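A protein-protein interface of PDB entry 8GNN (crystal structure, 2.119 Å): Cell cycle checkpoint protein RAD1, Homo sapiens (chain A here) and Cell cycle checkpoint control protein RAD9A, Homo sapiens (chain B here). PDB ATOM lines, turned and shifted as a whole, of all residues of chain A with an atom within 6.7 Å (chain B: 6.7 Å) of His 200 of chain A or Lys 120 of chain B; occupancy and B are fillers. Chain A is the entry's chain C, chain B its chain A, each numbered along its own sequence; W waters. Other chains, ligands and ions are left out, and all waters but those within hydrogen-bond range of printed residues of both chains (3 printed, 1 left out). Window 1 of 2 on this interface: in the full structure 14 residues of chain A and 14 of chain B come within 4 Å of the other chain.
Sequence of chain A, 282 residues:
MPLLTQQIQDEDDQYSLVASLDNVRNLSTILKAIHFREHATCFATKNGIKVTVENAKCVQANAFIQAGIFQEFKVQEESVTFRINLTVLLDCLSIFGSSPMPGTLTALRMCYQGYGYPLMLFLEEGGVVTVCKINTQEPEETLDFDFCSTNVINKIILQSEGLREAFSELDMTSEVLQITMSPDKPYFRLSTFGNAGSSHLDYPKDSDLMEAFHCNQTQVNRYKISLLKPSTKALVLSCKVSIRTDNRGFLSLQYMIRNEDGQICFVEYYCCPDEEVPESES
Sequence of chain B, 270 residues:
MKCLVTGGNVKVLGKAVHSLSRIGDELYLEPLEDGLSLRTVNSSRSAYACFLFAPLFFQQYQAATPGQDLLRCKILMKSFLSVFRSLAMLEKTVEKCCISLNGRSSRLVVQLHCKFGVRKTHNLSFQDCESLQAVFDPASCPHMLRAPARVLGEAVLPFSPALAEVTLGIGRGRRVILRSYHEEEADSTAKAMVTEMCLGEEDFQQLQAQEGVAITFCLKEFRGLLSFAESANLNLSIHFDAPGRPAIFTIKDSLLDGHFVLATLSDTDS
OE1 of Gln 111 of chain B lies close to NE of Arg 119 of chain B (3.5 Å).
N of Leu 112 of chain B sits at hydrogen-bond distance from O of Lys 120 of chain B, 2.7 Å away.
OD1 of Asp 202 of chain A is in salt-bridge range of NE of Arg 189 of chain A, 2.7 Å away.
O of Leu 190 of chain A is in hydrogen-bond range of N of Leu 201 of chain A, 2.7 Å away.
OG of Ser 191 of chain A is in hydrogen-bond range of ND1 of His 200 of chain A (2.5 Å).
The side-chain hydroxyl (OG) of Ser 198 of chain A is in hydrogen-bond range of a ring nitrogen (NE2) of His 200 of chain A (3.0 Å).
Printed residues of chain A that touch a printed residue of chain B: Ser 198, Ser 199, His 200, Leu 201 and Asp 202.
Of the 13 printed residues of chain B, 6 touch a printed residue of chain A.
Along chain B the printed residues that touch a printed residue of chain A span positions 118 to 123.
Among the printed residues, 13 pairs touch across the chains.
Among the printed residues, no Asp or Glu carboxylate lies within 4 Å of a Lys or Arg side-chain nitrogen of the other chain.
His 200 of chain A touches four residues of chain B.
Of chain A, only Ser 199 and His 200 come within 4 Å of Lys 120 of chain B.
Printed residues of chain A within 4 Å of Arg 119 of chain B: His 200, Leu 201 and Asp 202.
Of the printed residues of chain B, Ser 199 of chain A touches Lys 120 (3.5 Å), Thr 121 (3.2 Å) and His 122 (3.7 Å).
Ser 191 of chain A touches none of the printed residues of chain B.
The nearest residue of chain A that does not touch Lys 120 of chain B is Leu 201 of chain A (4.04 Å).
The nearest printed residue of chain A that does not touch His 122 of chain B is His 200 of chain A (5.0 Å).
The backbone NH of Asp 202 of chain A lies within hydrogen-bond range of the backbone carbonyl oxygen of Arg 119 of chain B (2.9 Å).
The side-chain hydroxyl of Ser 199 of chain A sits at hydrogen-bond distance from the side-chain amino group of Lys 120 of chain B (3.5 Å).
O of Thr 121 of chain B is in hydrogen-bond range of N of His 200 of chain A, at 2.8 Å.
The backbone NH (N) of Asn 123 of chain B lies within hydrogen-bond range of the backbone carbonyl oxygen (O) of Ser 198 of chain A (2.7 Å).
Water W1 bridges the side-chain carboxylate of Asp 202 of chain A (2.9 Å) and the guanidinium group of Arg 119 of chain B (2.9 Å).
Water W2 bridges ND2 of Asn 123 of chain B (3.3 Å) and NE2 of His 200 of chain A (3.4 Å).
Water W3 bridges the backbone carbonyl oxygen of Ser 82 of chain B (3.4 Å) and the side-chain carboxylate of Glu 169 of chain A (3.4 Å).
Among the printed residues, pairs that only touch across the chains: Ser 198 of chain A with His 122 of chain B (3.6 Å), Ser 199 of chain A with Thr 121 of chain B (3.2 Å), Ser 199 of chain A with His 122 of chain B (3.7 Å), His 200 of chain A with Arg 119 of chain B (3.7 Å), His 200 of chain A with Lys 120 of chain B (3.3 Å), His 200 of chain A with Asn 123 of chain B (3.7 Å), Leu 201 of chain A with Val 118 of chain B (3.8 Å), Leu 201 of chain A with Arg 119 of chain B (3.8 Å) and Asp 202 of chain A with Val 118 of chain B (3.4 Å).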
ATOM      1  N   ALA A 166     -17.353   3.875 -20.323  1.00  0.00           N
ATOM      2  CA  ALA A 166     -18.132   5.088 -20.125  1.00  0.00           C
ATOM      3  C   ALA A 166     -19.600   4.750 -19.865  1.00  0.00           C
ATOM      4  O   ALA A 166     -20.283   5.459 -19.125  1.00  0.00           O
ATOM      5  CB  ALA A 166     -17.997   6.011 -21.324  1.00  0.00           C
ATOM      6  N   GLU A 169     -20.451   3.159 -16.332  1.00  0.00           N
ATOM      7  CA  GLU A 169     -20.447   4.084 -15.229  1.00  0.00           C
ATOM      8  C   GLU A 169     -21.665   4.962 -15.109  1.00  0.00           C
ATOM      9  O   GLU A 169     -21.773   5.716 -14.178  1.00  0.00           O
ATOM     10  CB  GLU A 169     -19.224   4.962 -15.302  1.00  0.00           C
ATOM     11  CG  GLU A 169     -18.230   4.645 -14.225  1.00  0.00           C
ATOM     12  CD  GLU A 169     -16.901   5.223 -14.531  1.00  0.00           C
ATOM     13  OE1 GLU A 169     -16.864   6.281 -15.171  1.00  0.00           O
ATOM     14  OE2 GLU A 169     -15.905   4.611 -14.142  1.00  0.00           O
ATOM     15  N   LEU A 170     -22.587   4.889 -16.041  1.00  0.00           N
ATOM     16  CA  LEU A 170     -23.718   5.801 -15.951  1.00  0.00           C
ATOM     17  C   LEU A 170     -24.475   5.646 -14.641  1.00  0.00           C
ATOM     18  O   LEU A 170     -24.759   4.533 -14.187  1.00  0.00           O
ATOM     19  CB  LEU A 170     -24.676   5.583 -17.120  1.00  0.00           C
ATOM     20  CG  LEU A 170     -24.089   5.674 -18.530  1.00  0.00           C
ATOM     21  CD1 LEU A 170     -24.695   4.611 -19.439  1.00  0.00           C
ATOM     22  CD2 LEU A 170     -24.271   7.064 -19.122  1.00  0.00           C
ATOM     23  N   ASP A 171     -24.825   6.790 -14.069  1.00  0.00           N
ATOM     24  CA  ASP A 171     -25.462   6.876 -12.765  1.00  0.00           C
ATOM     25  C   ASP A 171     -26.714   6.005 -12.665  1.00  0.00           C
ATOM     26  O   ASP A 171     -27.729   6.285 -13.300  1.00  0.00           O
ATOM     27  CB  ASP A 171     -25.798   8.339 -12.468  1.00  0.00           C
ATOM     28  CG  ASP A 171     -26.448   8.527 -11.120  1.00  0.00           C
ATOM     29  OD1 ASP A 171     -26.251   7.669 -10.235  1.00  0.00           O
ATOM     30  OD2 ASP A 171     -27.150   9.542 -10.944  1.00  0.00           O
ATOM     31  N   GLN A 178     -31.533   8.950 -20.960  1.00  0.00           N
ATOM     32  CA  GLN A 178     -32.027   9.738 -22.080  1.00  0.00           C
ATOM     33  C   GLN A 178     -31.051   9.706 -23.249  1.00  0.00           C
ATOM     34  O   GLN A 178     -29.911  10.157 -23.132  1.00  0.00           O
ATOM     35  CB  GLN A 178     -32.286  11.181 -21.647  1.00  0.00           C
ATOM     36  CG  GLN A 178     -32.958  12.031 -22.709  1.00  0.00           C
ATOM     37  CD  GLN A 178     -33.374  13.390 -22.188  1.00  0.00           C
ATOM     38  OE1 GLN A 178     -34.488  13.563 -21.692  1.00  0.00           O
ATOM     39  NE2 GLN A 178     -32.480  14.366 -22.295  1.00  0.00           N
ATOM     40  N   ARG A 189     -25.844  11.954 -27.650  1.00  0.00           N
ATOM     41  CA  ARG A 189     -25.745  12.215 -26.218  1.00  0.00           C
ATOM     42  C   ARG A 189     -26.482  11.186 -25.365  1.00  0.00           C
ATOM     43  O   ARG A 189     -27.632  10.842 -25.634  1.00  0.00           O
ATOM     44  CB  ARG A 189     -26.277  13.613 -25.898  1.00  0.00           C
ATOM     45  CG  ARG A 189     -26.526  13.847 -24.414  1.00  0.00           C
ATOM     46  CD  ARG A 189     -26.879  15.294 -24.121  1.00  0.00           C
ATOM     47  NE  ARG A 189     -25.734  16.180 -24.303  1.00  0.00           N
ATOM     48  CZ  ARG A 189     -25.743  17.478 -24.016  1.00  0.00           C
ATOM     49  NH1 ARG A 189     -26.840  18.044 -23.531  1.00  0.00           N
ATOM     50  NH2 ARG A 189     -24.654  18.209 -24.212  1.00  0.00           N
ATOM     51  N   LEU A 190     -25.800  10.702 -24.331  1.00  0.00           N
ATOM     52  CA  LEU A 190     -26.422   9.870 -23.310  1.00  0.00           C
ATOM     53  C   LEU A 190     -26.509  10.659 -22.009  1.00  0.00           C
ATOM     54  O   LEU A 190     -25.493  11.127 -21.492  1.00  0.00           O
ATOM     55  CB  LEU A 190     -25.632   8.577 -23.100  1.00  0.00           C
ATOM     56  CG  LEU A 190     -25.430   7.692 -24.331  1.00  0.00           C
ATOM     57  CD1 LEU A 190     -24.550   6.499 -23.993  1.00  0.00           C
ATOM     58  CD2 LEU A 190     -26.770   7.234 -24.883  1.00  0.00           C
ATOM     59  N   SER A 191     -27.720  10.814 -21.486  1.00  0.00           N
ATOM     60  CA  SER A 191     -27.926  11.625 -20.290  1.00  0.00           C
ATOM     61  C   SER A 191     -28.575  10.842 -19.154  1.00  0.00           C
ATOM     62  O   SER A 191     -29.439   9.995 -19.381  1.00  0.00           O
ATOM     63  CB  SER A 191     -28.782  12.849 -20.623  1.00  0.00           C
ATOM     64  OG  SER A 191     -28.127  13.692 -21.553  1.00  0.00           O
ATOM     65  N   THR A 192     -28.145  11.136 -17.931  1.00  0.00           N
ATOM     66  CA  THR A 192     -28.768  10.578 -16.738  1.00  0.00           C
ATOM     67  C   THR A 192     -29.118  11.700 -15.767  1.00  0.00           C
ATOM     68  O   THR A 192     -28.487  12.757 -15.773  1.00  0.00           O
ATOM     69  CB  THR A 192     -27.856   9.553 -16.032  1.00  0.00           C
ATOM     70  OG1 THR A 192     -26.624  10.180 -15.658  1.00  0.00           O
ATOM     71  CG2 THR A 192     -27.567   8.371 -16.947  1.00  0.00           C
ATOM     72  N   PHE A 193     -30.131  11.468 -14.939  1.00  0.00           N
ATOM     73  CA  PHE A 193     -30.589  12.476 -13.991  1.00  0.00           C
ATOM     74  C   PHE A 193     -30.799  11.859 -12.614  1.00  0.00           C
ATOM     75  O   PHE A 193     -31.913  11.471 -12.262  1.00  0.00           O
ATOM     76  CB  PHE A 193     -31.885  13.128 -14.480  1.00  0.00           C
ATOM     77  CG  PHE A 193     -31.819  13.624 -15.899  1.00  0.00           C
ATOM     78  CD1 PHE A 193     -32.131  12.786 -16.957  1.00  0.00           C
ATOM     79  CD2 PHE A 193     -31.447  14.930 -16.174  1.00  0.00           C
ATOM     80  CE1 PHE A 193     -32.071  13.237 -18.261  1.00  0.00           C
ATOM     81  CE2 PHE A 193     -31.387  15.389 -17.477  1.00  0.00           C
ATOM     82  CZ  PHE A 193     -31.699  14.540 -18.522  1.00  0.00           C
ATOM     83  N   SER A 198     -27.280  16.336 -12.905  1.00  0.00           N
ATOM     84  CA  SER A 198     -27.309  15.957 -14.311  1.00  0.00           C
ATOM     85  C   SER A 198     -25.951  15.459 -14.795  1.00  0.00           C
ATOM     86  O   SER A 198     -24.909  15.868 -14.283  1.00  0.00           O
ATOM     87  CB  SER A 198     -27.767  17.140 -15.168  1.00  0.00           C
ATOM     88  OG  SER A 198     -27.484  16.918 -16.537  1.00  0.00           O
ATOM     89  N   SER A 199     -25.972  14.575 -15.787  1.00  0.00           N
ATOM     90  CA  SER A 199     -24.746  14.030 -16.360  1.00  0.00           C
ATOM     91  C   SER A 199     -24.927  13.721 -17.843  1.00  0.00           C
ATOM     92  O   SER A 199     -25.821  12.965 -18.219  1.00  0.00           O
ATOM     93  CB  SER A 199     -24.316  12.771 -15.607  1.00  0.00           C
ATOM     94  OG  SER A 199     -23.144  12.214 -16.174  1.00  0.00           O
ATOM     95  N   HIS A 200     -24.076  14.307 -18.680  1.00  0.00           N
ATOM     96  CA  HIS A 200     -24.179  14.121 -20.124  1.00  0.00           C
ATOM     97  C   HIS A 200     -22.923  13.485 -20.715  1.00  0.00           C
ATOM     98  O   HIS A 200     -21.804  13.888 -20.402  1.00  0.00           O
ATOM     99  CB  HIS A 200     -24.451  15.459 -20.818  1.00  0.00           C
ATOM    100  CG  HIS A 200     -25.675  16.161 -20.322  1.00  0.00           C
ATOM    101  ND1 HIS A 200     -26.951  15.703 -20.577  1.00  0.00           N
ATOM    102  CD2 HIS A 200     -25.821  17.291 -19.591  1.00  0.00           C
ATOM    103  CE1 HIS A 200     -27.828  16.520 -20.022  1.00  0.00           C
ATOM    104  NE2 HIS A 200     -27.169  17.491 -19.417  1.00  0.00           N
ATOM    105  N   LEU A 201     -23.124  12.493 -21.575  1.00  0.00           N
ATOM    106  CA  LEU A 201     -22.029  11.847 -22.290  1.00  0.00           C
ATOM    107  C   LEU A 201     -22.193  12.078 -23.789  1.00  0.00           C
ATOM    108  O   LEU A 201     -23.125  11.560 -24.403  1.00  0.00           O
ATOM    109  CB  LEU A 201     -21.989  10.352 -21.974  1.00  0.00           C
ATOM    110  CG  LEU A 201     -20.817   9.543 -22.532  1.00  0.00           C
ATOM    111  CD1 LEU A 201     -19.489  10.130 -22.077  1.00  0.00           C
ATOM    112  CD2 LEU A 201     -20.936   8.086 -22.115  1.00  0.00           C
ATOM    113  N   ASP A 202     -21.287  12.855 -24.377  1.00  0.00           N
ATOM    114  CA  ASP A 202     -21.438  13.276 -25.767  1.00  0.00           C
ATOM    115  C   ASP A 202     -20.398  12.672 -26.706  1.00  0.00           C
ATOM    116  O   ASP A 202     -19.204  12.656 -26.409  1.00  0.00           O
ATOM    117  CB  ASP A 202     -21.380  14.802 -25.862  1.00  0.00           C
ATOM    118  CG  ASP A 202     -22.515  15.476 -25.121  1.00  0.00           C
ATOM    119  OD1 ASP A 202     -23.484  14.778 -24.758  1.00  0.00           O
ATOM    120  OD2 ASP A 202     -22.443  16.704 -24.907  1.00  0.00           O
ATOM    121  N   SER B  82     -17.732  10.330  -7.541  1.00  0.00           N
ATOM    122  CA  SER B  82     -18.305   9.619  -8.680  1.00  0.00           C
ATOM    123  C   SER B  82     -17.704  10.085 -10.003  1.00  0.00           C
ATOM    124  O   SER B  82     -17.462   9.278 -10.901  1.00  0.00           O
ATOM    125  CB  SER B  82     -19.825   9.798  -8.705  1.00  0.00           C
ATOM    126  OG  SER B  82     -20.393   9.184  -9.849  1.00  0.00           O
ATOM    127  N   VAL B  83     -17.461  11.387 -10.113  1.00  0.00           N
ATOM    128  CA  VAL B  83     -16.878  11.966 -11.319  1.00  0.00           C
ATOM    129  C   VAL B  83     -15.472  11.418 -11.565  1.00  0.00           C
ATOM    130  O   VAL B  83     -15.077  11.176 -12.706  1.00  0.00           O
ATOM    131  CB  VAL B  83     -16.827  13.507 -11.226  1.00  0.00           C
ATOM    132  CG1 VAL B  83     -16.122  14.102 -12.437  1.00  0.00           C
ATOM    133  CG2 VAL B  83     -18.233  14.073 -11.088  1.00  0.00           C
ATOM    134  N   VAL B 110     -18.591  20.083 -13.929  1.00  0.00           N
ATOM    135  CA  VAL B 110     -17.323  19.399 -14.140  1.00  0.00           C
ATOM    136  C   VAL B 110     -17.313  18.732 -15.510  1.00  0.00           C
ATOM    137  O   VAL B 110     -18.034  17.762 -15.744  1.00  0.00           O
ATOM    138  CB  VAL B 110     -17.048  18.340 -13.057  1.00  0.00           C
ATOM    139  CG1 VAL B 110     -15.690  17.694 -13.289  1.00  0.00           C
ATOM    140  CG2 VAL B 110     -17.116  18.965 -11.674  1.00  0.00           C
ATOM    141  N   GLN B 111     -16.500  19.265 -16.416  1.00  0.00           N
ATOM    142  CA  GLN B 111     -16.381  18.702 -17.755  1.00  0.00           C
ATOM    143  C   GLN B 111     -15.107  17.889 -17.909  1.00  0.00           C
ATOM    144  O   GLN B 111     -14.016  18.356 -17.582  1.00  0.00           O
ATOM    145  CB  GLN B 111     -16.408  19.801 -18.815  1.00  0.00           C
ATOM    146  CG  GLN B 111     -17.695  20.594 -18.879  1.00  0.00           C
ATOM    147  CD  GLN B 111     -17.702  21.571 -20.036  1.00  0.00           C
ATOM    148  OE1 GLN B 111     -17.700  21.170 -21.201  1.00  0.00           O
ATOM    149  NE2 GLN B 111     -17.696  22.860 -19.723  1.00  0.00           N
ATOM    150  N   LEU B 112     -15.251  16.670 -18.413  1.00  0.00           N
ATOM    151  CA  LEU B 112     -14.100  15.844 -18.739  1.00  0.00           C
ATOM    152  C   LEU B 112     -13.931  15.769 -20.251  1.00  0.00           C
ATOM    153  O   LEU B 112     -14.743  15.160 -20.947  1.00  0.00           O
ATOM    154  CB  LEU B 112     -14.250  14.443 -18.144  1.00  0.00           C
ATOM    155  CG  LEU B 112     -14.505  14.391 -16.637  1.00  0.00           C
ATOM    156  CD1 LEU B 112     -14.665  12.956 -16.162  1.00  0.00           C
ATOM    157  CD2 LEU B 112     -13.385  15.091 -15.881  1.00  0.00           C
ATOM    158  N   HIS B 113     -12.883  16.412 -20.753  1.00  0.00           N
ATOM    159  CA  HIS B 113     -12.561  16.349 -22.171  1.00  0.00           C
ATOM    160  C   HIS B 113     -11.754  15.087 -22.439  1.00  0.00           C
ATOM    161  O   HIS B 113     -10.603  14.972 -22.020  1.00  0.00           O
ATOM    162  CB  HIS B 113     -11.791  17.595 -22.611  1.00  0.00           C
ATOM    163  CG  HIS B 113     -12.537  18.873 -22.387  1.00  0.00           C
ATOM    164  ND1 HIS B 113     -13.417  19.393 -23.311  1.00  0.00           N
ATOM    165  CD2 HIS B 113     -12.541  19.732 -21.341  1.00  0.00           C
ATOM    166  CE1 HIS B 113     -13.928  20.518 -22.847  1.00  0.00           C
ATOM    167  NE2 HIS B 113     -13.413  20.748 -21.652  1.00  0.00           N
ATOM    168  N   CYS B 114     -12.371  14.135 -23.130  1.00  0.00           N
ATOM    169  CA  CYS B 114     -11.783  12.813 -23.291  1.00  0.00           C
ATOM    170  C   CYS B 114     -11.284  12.561 -24.708  1.00  0.00           C
ATOM    171  O   CYS B 114     -11.465  13.390 -25.601  1.00  0.00           O
ATOM    172  CB  CYS B 114     -12.801  11.742 -22.898  1.00  0.00           C
ATOM    173  SG  CYS B 114     -13.507  11.971 -21.247  1.00  0.00           S
ATOM    174  N   VAL B 118     -14.749  12.816 -27.228  1.00  0.00           N
ATOM    175  CA  VAL B 118     -15.802  12.531 -26.258  1.00  0.00           C
ATOM    176  C   VAL B 118     -15.756  13.523 -25.099  1.00  0.00           C
ATOM    177  O   VAL B 118     -14.689  13.803 -24.553  1.00  0.00           O
ATOM    178  CB  VAL B 118     -15.688  11.098 -25.708  1.00  0.00           C
ATOM    179  CG1 VAL B 118     -16.833  10.801 -24.749  1.00  0.00           C
ATOM    180  CG2 VAL B 118     -15.675  10.095 -26.850  1.00  0.00           C
ATOM    181  N   ARG B 119     -16.916  14.059 -24.733  1.00  0.00           N
ATOM    182  CA  ARG B 119     -17.002  14.993 -23.617  1.00  0.00           C
ATOM    183  C   ARG B 119     -18.040  14.528 -22.601  1.00  0.00           C
ATOM    184  O   ARG B 119     -19.186  14.246 -22.955  1.00  0.00           O
ATOM    185  CB  ARG B 119     -17.342  16.401 -24.115  1.00  0.00           C
ATOM    186  CG  ARG B 119     -17.134  17.493 -23.076  1.00  0.00           C
ATOM    187  CD  ARG B 119     -17.297  18.884 -23.675  1.00  0.00           C
ATOM    188  NE  ARG B 119     -18.699  19.240 -23.881  1.00  0.00           N
ATOM    189  CZ  ARG B 119     -19.109  20.410 -24.360  1.00  0.00           C
ATOM    190  NH1 ARG B 119     -18.223  21.342 -24.687  1.00  0.00           N
ATOM    191  NH2 ARG B 119     -20.403  20.650 -24.513  1.00  0.00           N
ATOM    192  N   LYS B 120     -17.629  14.438 -21.340  1.00  0.00           N
ATOM    193  CA  LYS B 120     -18.545  14.068 -20.268  1.00  0.00           C
ATOM    194  C   LYS B 120     -18.771  15.247 -19.330  1.00  0.00           C
ATOM    195  O   LYS B 120     -17.826  15.779 -18.746  1.00  0.00           O
ATOM    196  CB  LYS B 120     -18.014  12.861 -19.491  1.00  0.00           C
ATOM    197  CG  LYS B 120     -19.035  12.249 -18.543  1.00  0.00           C
ATOM    198  CD  LYS B 120     -18.543  10.932 -17.965  1.00  0.00           C
ATOM    199  CE  LYS B 120     -19.592  10.303 -17.063  1.00  0.00           C
ATOM    200  NZ  LYS B 120     -20.880  10.080 -17.777  1.00  0.00           N
ATOM    201  N   THR B 121     -20.028  15.652 -19.193  1.00  0.00           N
ATOM    202  CA  THR B 121     -20.374  16.825 -18.400  1.00  0.00           C
ATOM    203  C   THR B 121     -21.188  16.454 -17.168  1.00  0.00           C
ATOM    204  O   THR B 121     -22.225  15.801 -17.272  1.00  0.00           O
ATOM    205  CB  THR B 121     -21.169  17.848 -19.234  1.00  0.00           C
ATOM    206  OG1 THR B 121     -20.395  18.243 -20.373  1.00  0.00           O
ATOM    207  CG2 THR B 121     -21.502  19.077 -18.401  1.00  0.00           C
ATOM    208  N   HIS B 122     -20.711  16.873 -16.000  1.00  0.00           N
ATOM    209  CA  HIS B 122     -21.427  16.647 -14.752  1.00  0.00           C
ATOM    210  C   HIS B 122     -21.965  17.958 -14.190  1.00  0.00           C
ATOM    211  O   HIS B 122     -21.203  18.890 -13.931  1.00  0.00           O
ATOM    212  CB  HIS B 122     -20.521  15.969 -13.721  1.00  0.00           C
ATOM    213  CG  HIS B 122     -20.000  14.635 -14.155  1.00  0.00           C
ATOM    214  ND1 HIS B 122     -20.626  13.451 -13.831  1.00  0.00           N
ATOM    215  CD2 HIS B 122     -18.911  14.298 -14.886  1.00  0.00           C
ATOM    216  CE1 HIS B 122     -19.945  12.442 -14.344  1.00  0.00           C
ATOM    217  NE2 HIS B 122     -18.900  12.929 -14.989  1.00  0.00           N
ATOM    218  N   ASN B 123     -23.279  18.026 -14.010  1.00  0.00           N
ATOM    219  CA  ASN B 123     -23.907  19.190 -13.398  1.00  0.00           C
ATOM    220  C   ASN B 123     -24.254  18.901 -11.944  1.00  0.00           C
ATOM    221  O   ASN B 123     -25.345  18.419 -11.639  1.00  0.00           O
ATOM    222  CB  ASN B 123     -25.156  19.601 -14.177  1.00  0.00           C
ATOM    223  CG  ASN B 123     -24.850  19.953 -15.621  1.00  0.00           C
ATOM    224  OD1 ASN B 123     -23.980  20.778 -15.899  1.00  0.00           O
ATOM    225  ND2 ASN B 123     -25.561  19.321 -16.546  1.00  0.00           N
HETATM  226  O   HOH W   1     -20.546  18.348 -26.302  1.00  0.00           O
HETATM  227  O   HOH W   2     -25.656  20.560 -19.586  1.00  0.00           O
HETATM  228  O   HOH W   3     -18.628   8.980 -14.035  1.00  0.00           O
